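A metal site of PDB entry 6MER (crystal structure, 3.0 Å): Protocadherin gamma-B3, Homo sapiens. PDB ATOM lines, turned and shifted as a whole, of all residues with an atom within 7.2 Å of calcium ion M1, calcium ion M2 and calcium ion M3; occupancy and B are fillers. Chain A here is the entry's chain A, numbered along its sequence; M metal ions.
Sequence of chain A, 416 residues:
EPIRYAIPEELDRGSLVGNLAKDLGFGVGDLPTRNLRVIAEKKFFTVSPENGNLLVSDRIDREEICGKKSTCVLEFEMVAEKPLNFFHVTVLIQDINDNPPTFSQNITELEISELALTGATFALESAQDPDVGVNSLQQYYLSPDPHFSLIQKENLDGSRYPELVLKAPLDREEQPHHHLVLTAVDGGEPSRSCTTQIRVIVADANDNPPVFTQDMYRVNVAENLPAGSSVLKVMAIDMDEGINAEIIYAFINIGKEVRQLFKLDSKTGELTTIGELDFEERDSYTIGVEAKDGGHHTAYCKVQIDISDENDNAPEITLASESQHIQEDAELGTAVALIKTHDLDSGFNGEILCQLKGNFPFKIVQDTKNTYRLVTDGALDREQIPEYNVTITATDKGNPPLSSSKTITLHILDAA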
ATOM      1  N   GLU A 114      -1.380  37.116 -31.509  1.00  0.00           N
ATOM      2  CA  GLU A 114      -1.652  36.501 -32.805  1.00  0.00           C
ATOM      3  C   GLU A 114      -2.742  37.233 -33.578  1.00  0.00           C
ATOM      4  O   GLU A 114      -2.783  37.115 -34.813  1.00  0.00           O
ATOM      5  CB  GLU A 114      -2.057  35.038 -32.614  1.00  0.00           C
ATOM      6  CG  GLU A 114      -1.097  34.212 -31.785  1.00  0.00           C
ATOM      7  CD  GLU A 114      -1.535  32.768 -31.655  1.00  0.00           C
ATOM      8  OE1 GLU A 114      -2.053  32.213 -32.646  1.00  0.00           O
ATOM      9  OE2 GLU A 114      -1.368  32.181 -30.569  1.00  0.00           O
ATOM     10  N   LEU A 170       0.587  36.410 -37.667  1.00  0.00           N
ATOM     11  CA  LEU A 170       1.412  35.740 -36.658  1.00  0.00           C
ATOM     12  C   LEU A 170       0.667  34.551 -36.084  1.00  0.00           C
ATOM     13  O   LEU A 170      -0.486  34.679 -35.648  1.00  0.00           O
ATOM     14  CB  LEU A 170       1.792  36.709 -35.545  1.00  0.00           C
ATOM     15  CG  LEU A 170       2.787  37.824 -35.904  1.00  0.00           C
ATOM     16  CD1 LEU A 170       3.142  38.644 -34.683  1.00  0.00           C
ATOM     17  CD2 LEU A 170       4.035  37.233 -36.552  1.00  0.00           C
ATOM     18  N   ASP A 171       1.317  33.393 -36.080  1.00  0.00           N
ATOM     19  CA  ASP A 171       0.774  32.164 -35.514  1.00  0.00           C
ATOM     20  C   ASP A 171       1.767  31.650 -34.478  1.00  0.00           C
ATOM     21  O   ASP A 171       2.830  31.140 -34.849  1.00  0.00           O
ATOM     22  CB  ASP A 171       0.506  31.129 -36.601  1.00  0.00           C
ATOM     23  CG  ASP A 171      -0.246  29.910 -36.083  1.00  0.00           C
ATOM     24  OD1 ASP A 171      -0.595  29.890 -34.887  1.00  0.00           O
ATOM     25  OD2 ASP A 171      -0.489  28.985 -36.880  1.00  0.00           O
ATOM     26  N   ARG A 172       1.435  31.794 -33.204  1.00  0.00           N
ATOM     27  CA  ARG A 172       2.324  31.327 -32.146  1.00  0.00           C
ATOM     28  C   ARG A 172       2.491  29.815 -32.191  1.00  0.00           C
ATOM     29  O   ARG A 172       3.572  29.299 -31.865  1.00  0.00           O
ATOM     30  CB  ARG A 172       1.798  31.753 -30.779  1.00  0.00           C
ATOM     31  CG  ARG A 172       2.756  31.475 -29.624  1.00  0.00           C
ATOM     32  CD  ARG A 172       2.013  31.372 -28.306  1.00  0.00           C
ATOM     33  NE  ARG A 172       1.128  30.205 -28.269  1.00  0.00           N
ATOM     34  CZ  ARG A 172       1.495  29.005 -27.841  1.00  0.00           C
ATOM     35  NH1 ARG A 172       2.731  28.802 -27.411  1.00  0.00           N
ATOM     36  NH2 ARG A 172       0.630  27.999 -27.845  1.00  0.00           N
ATOM     37  N   GLU A 173       1.447  29.094 -32.597  1.00  0.00           N
ATOM     38  CA  GLU A 173       1.537  27.636 -32.714  1.00  0.00           C
ATOM     39  C   GLU A 173       2.468  27.191 -33.831  1.00  0.00           C
ATOM     40  O   GLU A 173       2.830  26.015 -33.876  1.00  0.00           O
ATOM     41  CB  GLU A 173       0.143  27.045 -32.930  1.00  0.00           C
ATOM     42  CG  GLU A 173      -0.763  27.088 -31.704  1.00  0.00           C
ATOM     43  CD  GLU A 173      -1.209  28.490 -31.334  1.00  0.00           C
ATOM     44  OE1 GLU A 173      -1.478  29.297 -32.250  1.00  0.00           O
ATOM     45  OE2 GLU A 173      -1.282  28.800 -30.123  1.00  0.00           O
ATOM     46  N   GLU A 174       2.852  28.100 -34.724  1.00  0.00           N
ATOM     47  CA  GLU A 174       3.830  27.816 -35.773  1.00  0.00           C
ATOM     48  C   GLU A 174       5.207  28.369 -35.462  1.00  0.00           C
ATOM     49  O   GLU A 174       6.217  27.709 -35.749  1.00  0.00           O
ATOM     50  CB  GLU A 174       3.334  28.375 -37.110  1.00  0.00           C
ATOM     51  CG  GLU A 174       4.274  28.147 -38.286  1.00  0.00           C
ATOM     52  CD  GLU A 174       4.347  26.689 -38.706  1.00  0.00           C
ATOM     53  OE1 GLU A 174       3.407  25.920 -38.376  1.00  0.00           O
ATOM     54  OE2 GLU A 174       5.331  26.306 -39.360  1.00  0.00           O
ATOM     55  N   ALA A 203       2.567  36.796 -28.580  1.00  0.00           N
ATOM     56  CA  ALA A 203       1.693  36.514 -27.456  1.00  0.00           C
ATOM     57  C   ALA A 203       0.564  35.581 -27.885  1.00  0.00           C
ATOM     58  O   ALA A 203       0.054  35.671 -29.005  1.00  0.00           O
ATOM     59  CB  ALA A 203       1.118  37.805 -26.884  1.00  0.00           C
ATOM     60  N   ASP A 204       0.178  34.681 -26.989  1.00  0.00           N
ATOM     61  CA  ASP A 204      -0.829  33.683 -27.308  1.00  0.00           C
ATOM     62  C   ASP A 204      -2.220  34.313 -27.353  1.00  0.00           C
ATOM     63  O   ASP A 204      -2.537  35.220 -26.583  1.00  0.00           O
ATOM     64  CB  ASP A 204      -0.812  32.543 -26.287  1.00  0.00           C
ATOM     65  CG  ASP A 204      -1.826  31.467 -26.598  1.00  0.00           C
ATOM     66  OD1 ASP A 204      -1.646  30.748 -27.599  1.00  0.00           O
ATOM     67  OD2 ASP A 204      -2.814  31.349 -25.844  1.00  0.00           O
ATOM     68  N   ALA A 205      -3.049  33.822 -28.276  1.00  0.00           N
ATOM     69  CA  ALA A 205      -4.434  34.233 -28.406  1.00  0.00           C
ATOM     70  C   ALA A 205      -5.307  32.992 -28.526  1.00  0.00           C
ATOM     71  O   ALA A 205      -4.951  32.045 -29.231  1.00  0.00           O
ATOM     72  CB  ALA A 205      -4.640  35.148 -29.611  1.00  0.00           C
ATOM     73  N   ASN A 206      -6.446  33.006 -27.838  1.00  0.00           N
ATOM     74  CA  ASN A 206      -7.353  31.860 -27.822  1.00  0.00           C
ATOM     75  C   ASN A 206      -8.066  31.774 -29.166  1.00  0.00           C
ATOM     76  O   ASN A 206      -9.206  32.219 -29.348  1.00  0.00           O
ATOM     77  CB  ASN A 206      -8.351  31.966 -26.672  1.00  0.00           C
ATOM     78  CG  ASN A 206      -9.248  30.757 -26.565  1.00  0.00           C
ATOM     79  OD1 ASN A 206     -10.370  30.743 -27.082  1.00  0.00           O
ATOM     80  ND2 ASN A 206      -8.771  29.725 -25.874  1.00  0.00           N
ATOM     81  N   ASP A 207      -7.374  31.168 -30.140  1.00  0.00           N
ATOM     82  CA  ASP A 207      -7.927  30.978 -31.480  1.00  0.00           C
ATOM     83  C   ASP A 207      -8.046  29.511 -31.862  1.00  0.00           C
ATOM     84  O   ASP A 207      -8.548  29.218 -32.960  1.00  0.00           O
ATOM     85  CB  ASP A 207      -7.075  31.719 -32.523  1.00  0.00           C
ATOM     86  CG  ASP A 207      -5.665  31.143 -32.634  1.00  0.00           C
ATOM     87  OD1 ASP A 207      -5.166  30.587 -31.639  1.00  0.00           O
ATOM     88  OD2 ASP A 207      -5.068  31.262 -33.721  1.00  0.00           O
ATOM     89  N   ASN A 208      -7.610  28.588 -31.010  1.00  0.00           N
ATOM     90  CA  ASN A 208      -7.711  27.161 -31.284  1.00  0.00           C
ATOM     91  C   ASN A 208      -8.669  26.516 -30.296  1.00  0.00           C
ATOM     92  O   ASN A 208      -8.318  26.315 -29.123  1.00  0.00           O
ATOM     93  CB  ASN A 208      -6.338  26.485 -31.199  1.00  0.00           C
ATOM     94  CG  ASN A 208      -5.410  26.916 -32.324  1.00  0.00           C
ATOM     95  OD1 ASN A 208      -5.580  27.987 -32.914  1.00  0.00           O
ATOM     96  ND2 ASN A 208      -4.419  26.087 -32.624  1.00  0.00           N
ATOM     97  N   PRO A 209      -9.897  26.187 -30.698  1.00  0.00           N
ATOM     98  CA  PRO A 209     -10.824  25.506 -29.791  1.00  0.00           C
ATOM     99  C   PRO A 209     -10.341  24.113 -29.457  1.00  0.00           C
ATOM    100  O   PRO A 209      -9.495  23.548 -30.174  1.00  0.00           O
ATOM    101  CB  PRO A 209     -12.144  25.468 -30.590  1.00  0.00           C
ATOM    102  CG  PRO A 209     -11.984  26.510 -31.654  1.00  0.00           C
ATOM    103  CD  PRO A 209     -10.518  26.517 -31.984  1.00  0.00           C
ATOM    104  N   PRO A 210     -10.845  23.509 -28.372  1.00  0.00           N
ATOM    105  CA  PRO A 210     -10.458  22.132 -28.058  1.00  0.00           C
ATOM    106  C   PRO A 210     -10.905  21.162 -29.138  1.00  0.00           C
ATOM    107  O   PRO A 210     -11.912  21.382 -29.819  1.00  0.00           O
ATOM    108  CB  PRO A 210     -11.173  21.863 -26.726  1.00  0.00           C
ATOM    109  CG  PRO A 210     -11.420  23.221 -26.140  1.00  0.00           C
ATOM    110  CD  PRO A 210     -11.676  24.116 -27.311  1.00  0.00           C
ATOM    111  N   ILE A 237      -7.346  18.139 -27.053  1.00  0.00           N
ATOM    112  CA  ILE A 237      -6.066  18.787 -27.323  1.00  0.00           C
ATOM    113  C   ILE A 237      -6.322  20.259 -27.609  1.00  0.00           C
ATOM    114  O   ILE A 237      -7.153  20.603 -28.462  1.00  0.00           O
ATOM    115  CB  ILE A 237      -5.345  18.112 -28.500  1.00  0.00           C
ATOM    116  CG1 ILE A 237      -4.973  16.670 -28.150  1.00  0.00           C
ATOM    117  CG2 ILE A 237      -4.103  18.906 -28.880  1.00  0.00           C
ATOM    118  CD1 ILE A 237      -4.035  16.553 -26.980  1.00  0.00           C
ATOM    119  N   ASP A 238      -5.610  21.124 -26.889  1.00  0.00           N
ATOM    120  CA  ASP A 238      -5.685  22.570 -27.088  1.00  0.00           C
ATOM    121  C   ASP A 238      -4.265  23.075 -27.344  1.00  0.00           C
ATOM    122  O   ASP A 238      -3.428  23.058 -26.443  1.00  0.00           O
ATOM    123  CB  ASP A 238      -6.302  23.256 -25.868  1.00  0.00           C
ATOM    124  CG  ASP A 238      -6.853  24.633 -26.194  1.00  0.00           C
ATOM    125  OD1 ASP A 238      -6.219  25.359 -26.988  1.00  0.00           O
ATOM    126  OD2 ASP A 238      -7.924  24.984 -25.657  1.00  0.00           O
ATOM    127  N   MET A 239      -4.013  23.516 -28.580  1.00  0.00           N
ATOM    128  CA  MET A 239      -2.671  23.910 -29.002  1.00  0.00           C
ATOM    129  C   MET A 239      -2.246  25.268 -28.472  1.00  0.00           C
ATOM    130  O   MET A 239      -1.125  25.697 -28.763  1.00  0.00           O
ATOM    131  CB  MET A 239      -2.599  23.912 -30.528  1.00  0.00           C
ATOM    132  CG  MET A 239      -2.886  22.561 -31.176  1.00  0.00           C
ATOM    133  SD  MET A 239      -1.687  21.307 -30.705  1.00  0.00           S
ATOM    134  CE  MET A 239      -0.169  22.031 -31.325  1.00  0.00           C
ATOM    135  N   ASP A 240      -3.088  25.954 -27.691  1.00  0.00           N
ATOM    136  CA  ASP A 240      -2.748  27.280 -27.192  1.00  0.00           C
ATOM    137  C   ASP A 240      -1.817  27.184 -25.984  1.00  0.00           C
ATOM    138  O   ASP A 240      -1.209  26.144 -25.732  1.00  0.00           O
ATOM    139  CB  ASP A 240      -4.012  28.060 -26.845  1.00  0.00           C
ATOM    140  CG  ASP A 240      -4.860  28.353 -28.055  1.00  0.00           C
ATOM    141  OD1 ASP A 240      -4.317  28.397 -29.181  1.00  0.00           O
ATOM    142  OD2 ASP A 240      -6.086  28.556 -27.890  1.00  0.00           O
ATOM    143  N   GLU A 241      -1.699  28.283 -25.232  1.00  0.00           N
ATOM    144  CA  GLU A 241      -0.753  28.375 -24.133  1.00  0.00           C
ATOM    145  C   GLU A 241      -1.442  28.948 -22.900  1.00  0.00           C
ATOM    146  O   GLU A 241      -2.184  29.930 -22.992  1.00  0.00           O
ATOM    147  CB  GLU A 241       0.445  29.252 -24.505  1.00  0.00           C
ATOM    148  CG  GLU A 241       1.415  29.520 -23.370  1.00  0.00           C
ATOM    149  CD  GLU A 241       2.497  30.508 -23.737  1.00  0.00           C
ATOM    150  OE1 GLU A 241       2.547  30.922 -24.913  1.00  0.00           O
ATOM    151  OE2 GLU A 241       3.284  30.892 -22.842  1.00  0.00           O
ATOM    152  N   ILE A 243      -3.849  29.752 -19.953  1.00  0.00           N
ATOM    153  CA  ILE A 243      -5.282  29.650 -19.682  1.00  0.00           C
ATOM    154  C   ILE A 243      -6.046  29.258 -20.938  1.00  0.00           C
ATOM    155  O   ILE A 243      -7.086  28.580 -20.847  1.00  0.00           O
ATOM    156  CB  ILE A 243      -5.799  30.981 -19.089  1.00  0.00           C
ATOM    157  CG1 ILE A 243      -7.295  30.917 -18.813  1.00  0.00           C
ATOM    158  CG2 ILE A 243      -5.466  32.143 -20.026  1.00  0.00           C
ATOM    159  CD1 ILE A 243      -7.690  29.843 -17.818  1.00  0.00           C
ATOM    160  N   ASN A 244      -5.546  29.632 -22.117  1.00  0.00           N
ATOM    161  CA  ASN A 244      -6.202  29.282 -23.368  1.00  0.00           C
ATOM    162  C   ASN A 244      -6.026  27.812 -23.739  1.00  0.00           C
ATOM    163  O   ASN A 244      -6.498  27.401 -24.804  1.00  0.00           O
ATOM    164  CB  ASN A 244      -5.681  30.172 -24.491  1.00  0.00           C
ATOM    165  CG  ASN A 244      -5.846  31.643 -24.198  1.00  0.00           C
ATOM    166  OD1 ASN A 244      -6.763  32.044 -23.478  1.00  0.00           O
ATOM    167  ND2 ASN A 244      -4.974  32.468 -24.763  1.00  0.00           N
ATOM    168  N   ALA A 245      -5.360  27.013 -22.895  1.00  0.00           N
ATOM    169  CA  ALA A 245      -5.180  25.599 -23.150  1.00  0.00           C
ATOM    170  C   ALA A 245      -5.723  24.697 -22.044  1.00  0.00           C
ATOM    171  O   ALA A 245      -5.825  23.486 -22.256  1.00  0.00           O
ATOM    172  CB  ALA A 245      -3.701  25.277 -23.375  1.00  0.00           C
ATOM    173  N   GLU A 246      -6.048  25.249 -20.878  1.00  0.00           N
ATOM    174  CA  GLU A 246      -6.605  24.454 -19.791  1.00  0.00           C
ATOM    175  C   GLU A 246      -8.049  24.074 -20.133  1.00  0.00           C
ATOM    176  O   GLU A 246      -8.872  24.946 -20.401  1.00  0.00           O
ATOM    177  CB  GLU A 246      -6.545  25.221 -18.485  1.00  0.00           C
ATOM    178  CG  GLU A 246      -5.127  25.593 -18.050  1.00  0.00           C
ATOM    179  CD  GLU A 246      -5.108  26.450 -16.799  1.00  0.00           C
ATOM    180  OE1 GLU A 246      -6.197  26.845 -16.324  1.00  0.00           O
ATOM    181  OE2 GLU A 246      -3.998  26.728 -16.294  1.00  0.00           O
ATOM    182  N   ILE A 247      -8.332  22.776 -20.112  1.00  0.00           N
ATOM    183  CA  ILE A 247      -9.618  22.241 -20.544  1.00  0.00           C
ATOM    184  C   ILE A 247     -10.355  21.655 -19.350  1.00  0.00           C
ATOM    185  O   ILE A 247      -9.756  20.971 -18.516  1.00  0.00           O
ATOM    186  CB  ILE A 247      -9.431  21.180 -21.642  1.00  0.00           C
ATOM    187  CG1 ILE A 247      -8.531  21.718 -22.760  1.00  0.00           C
ATOM    188  CG2 ILE A 247     -10.779  20.740 -22.208  1.00  0.00           C
ATOM    189  CD1 ILE A 247      -8.152  20.690 -23.786  1.00  0.00           C
ATOM    190  N   ASP A 293     -12.502  25.858 -22.491  1.00  0.00           N
ATOM    191  CA  ASP A 293     -11.237  26.429 -22.056  1.00  0.00           C
ATOM    192  C   ASP A 293     -11.478  27.809 -21.425  1.00  0.00           C
ATOM    193  O   ASP A 293     -12.619  28.200 -21.146  1.00  0.00           O
ATOM    194  CB  ASP A 293     -10.239  26.504 -23.215  1.00  0.00           C
ATOM    195  CG  ASP A 293     -10.781  27.299 -24.398  1.00  0.00           C
ATOM    196  OD1 ASP A 293     -11.974  27.670 -24.373  1.00  0.00           O
ATOM    197  OD2 ASP A 293     -10.001  27.556 -25.337  1.00  0.00           O
ATOM    198  N   GLY A 294     -10.384  28.547 -21.213  1.00  0.00           N
ATOM    199  CA  GLY A 294     -10.498  29.874 -20.643  1.00  0.00           C
ATOM    200  C   GLY A 294     -11.160  30.876 -21.579  1.00  0.00           C
ATOM    201  O   GLY A 294     -11.836  31.797 -21.128  1.00  0.00           O
ATOM    202  N   GLY A 295     -10.960  30.703 -22.891  1.00  0.00           N
ATOM    203  CA  GLY A 295     -11.556  31.565 -23.884  1.00  0.00           C
ATOM    204  C   GLY A 295     -12.986  31.242 -24.231  1.00  0.00           C
ATOM    205  O   GLY A 295     -13.509  31.771 -25.224  1.00  0.00           O
ATOM    206  N   HIS A 297     -14.237  28.740 -25.603  1.00  0.00           N
ATOM    207  CA  HIS A 297     -14.411  27.943 -26.804  1.00  0.00           C
ATOM    208  C   HIS A 297     -14.854  26.530 -26.421  1.00  0.00           C
ATOM    209  O   HIS A 297     -14.193  25.859 -25.627  1.00  0.00           O
ATOM    210  CB  HIS A 297     -13.113  27.899 -27.612  1.00  0.00           C
ATOM    211  CG  HIS A 297     -12.951  29.056 -28.549  1.00  0.00           C
ATOM    212  ND1 HIS A 297     -11.919  29.129 -29.464  1.00  0.00           N
ATOM    213  CD2 HIS A 297     -13.686  30.173 -28.714  1.00  0.00           C
ATOM    214  CE1 HIS A 297     -12.022  30.250 -30.151  1.00  0.00           C
ATOM    215  NE2 HIS A 297     -13.089  30.903 -29.720  1.00  0.00           N
HETATM  216 CA    CA M   1      -3.075  30.540 -29.898  1.00  0.00          CA
HETATM  217 CA    CA M   2      -7.938  27.310 -26.865  1.00  0.00          CA
HETATM  218 CA    CA M   3      -2.831  30.334 -34.077  1.00  0.00          CA
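OD1 of Asp 207 lies close to OD1 of Asn 208, 2.9 Å away.
The backbone carbonyl oxygen (O) of Asp 240 sits close to the guanidinium group (NH2) of Arg 172 (3.4 Å).
The side-chain carboxylate (OE2) of Glu 114 sits close to the guanidinium group (NE) of Arg 172, at 3.9 Å.
N of Glu 114 sits at hydrogen-bond distance from O of Ala 203.
ND2 of Asn 244 sits at hydrogen-bond distance from OD2 of Asp 204, 2.7 Å away.
The backbone NH (N) of His 297 sits at hydrogen-bond distance from the side-chain carboxylate (OD1) of Asp 293, at 2.8 Å.
The side-chain carboxylate (OD1) of Asp 204 lies close to the guanidinium group (NE) of Arg 172.
The side-chain carboxylate of Asp 204 lies within hydrogen-bond range of the backbone NH of Glu 241 (3.3 Å).
The nearest printed residue that does not touch calcium ion M2 is Pro 209 (4.4 Å).
Within 4 Å of calcium ion M3: Glu 114, Asp 171, Glu 173, Asp 207 and Asn 208.
Along chain A the residues within 4 Å of calcium ion M3 span positions 114 to 208.
The nearest printed residue that does not touch calcium ion M3 is Arg 172 (4.6 Å).
Calcium ion M1 is bound by OE2 of Glu 114 (2.5 Å), O of Ala 205 (2.5 Å), OE2 of Glu 173 (2.5 Å), OD1 of Asp 240 (2.6 Å), OD1 of Asp 204 (2.7 Å) and OD1 of Asp 207 (2.7 Å).
Calcium ion M1 has six donor atoms within binding distance.
Slightly farther from calcium ion M1 lies OE1 of Glu 173 (3.1 Å).
Calcium ion M2 is bound by OD2 of Asp 240, O of Asn 208, O of Asn 244, OD2 of Asp 293, OD1 of Asp 238, OD2 of Asp 238 and ND2 of Asn 206.
The side-chain carboxylate (OD1) of Asp 171 binds calcium ion M3, 2.4 Å away.
OD2 of Asp 207 is bound to calcium ion M3, at 2.4 Å.
Calcium ion M3 is bound by OE1 of Glu 114 (2.5 Å).
The side-chain carboxylate (OE1) of Glu 173 binds calcium ion M3 (2.5 Å).
Calcium ion M3 has four donor atoms within binding distance.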
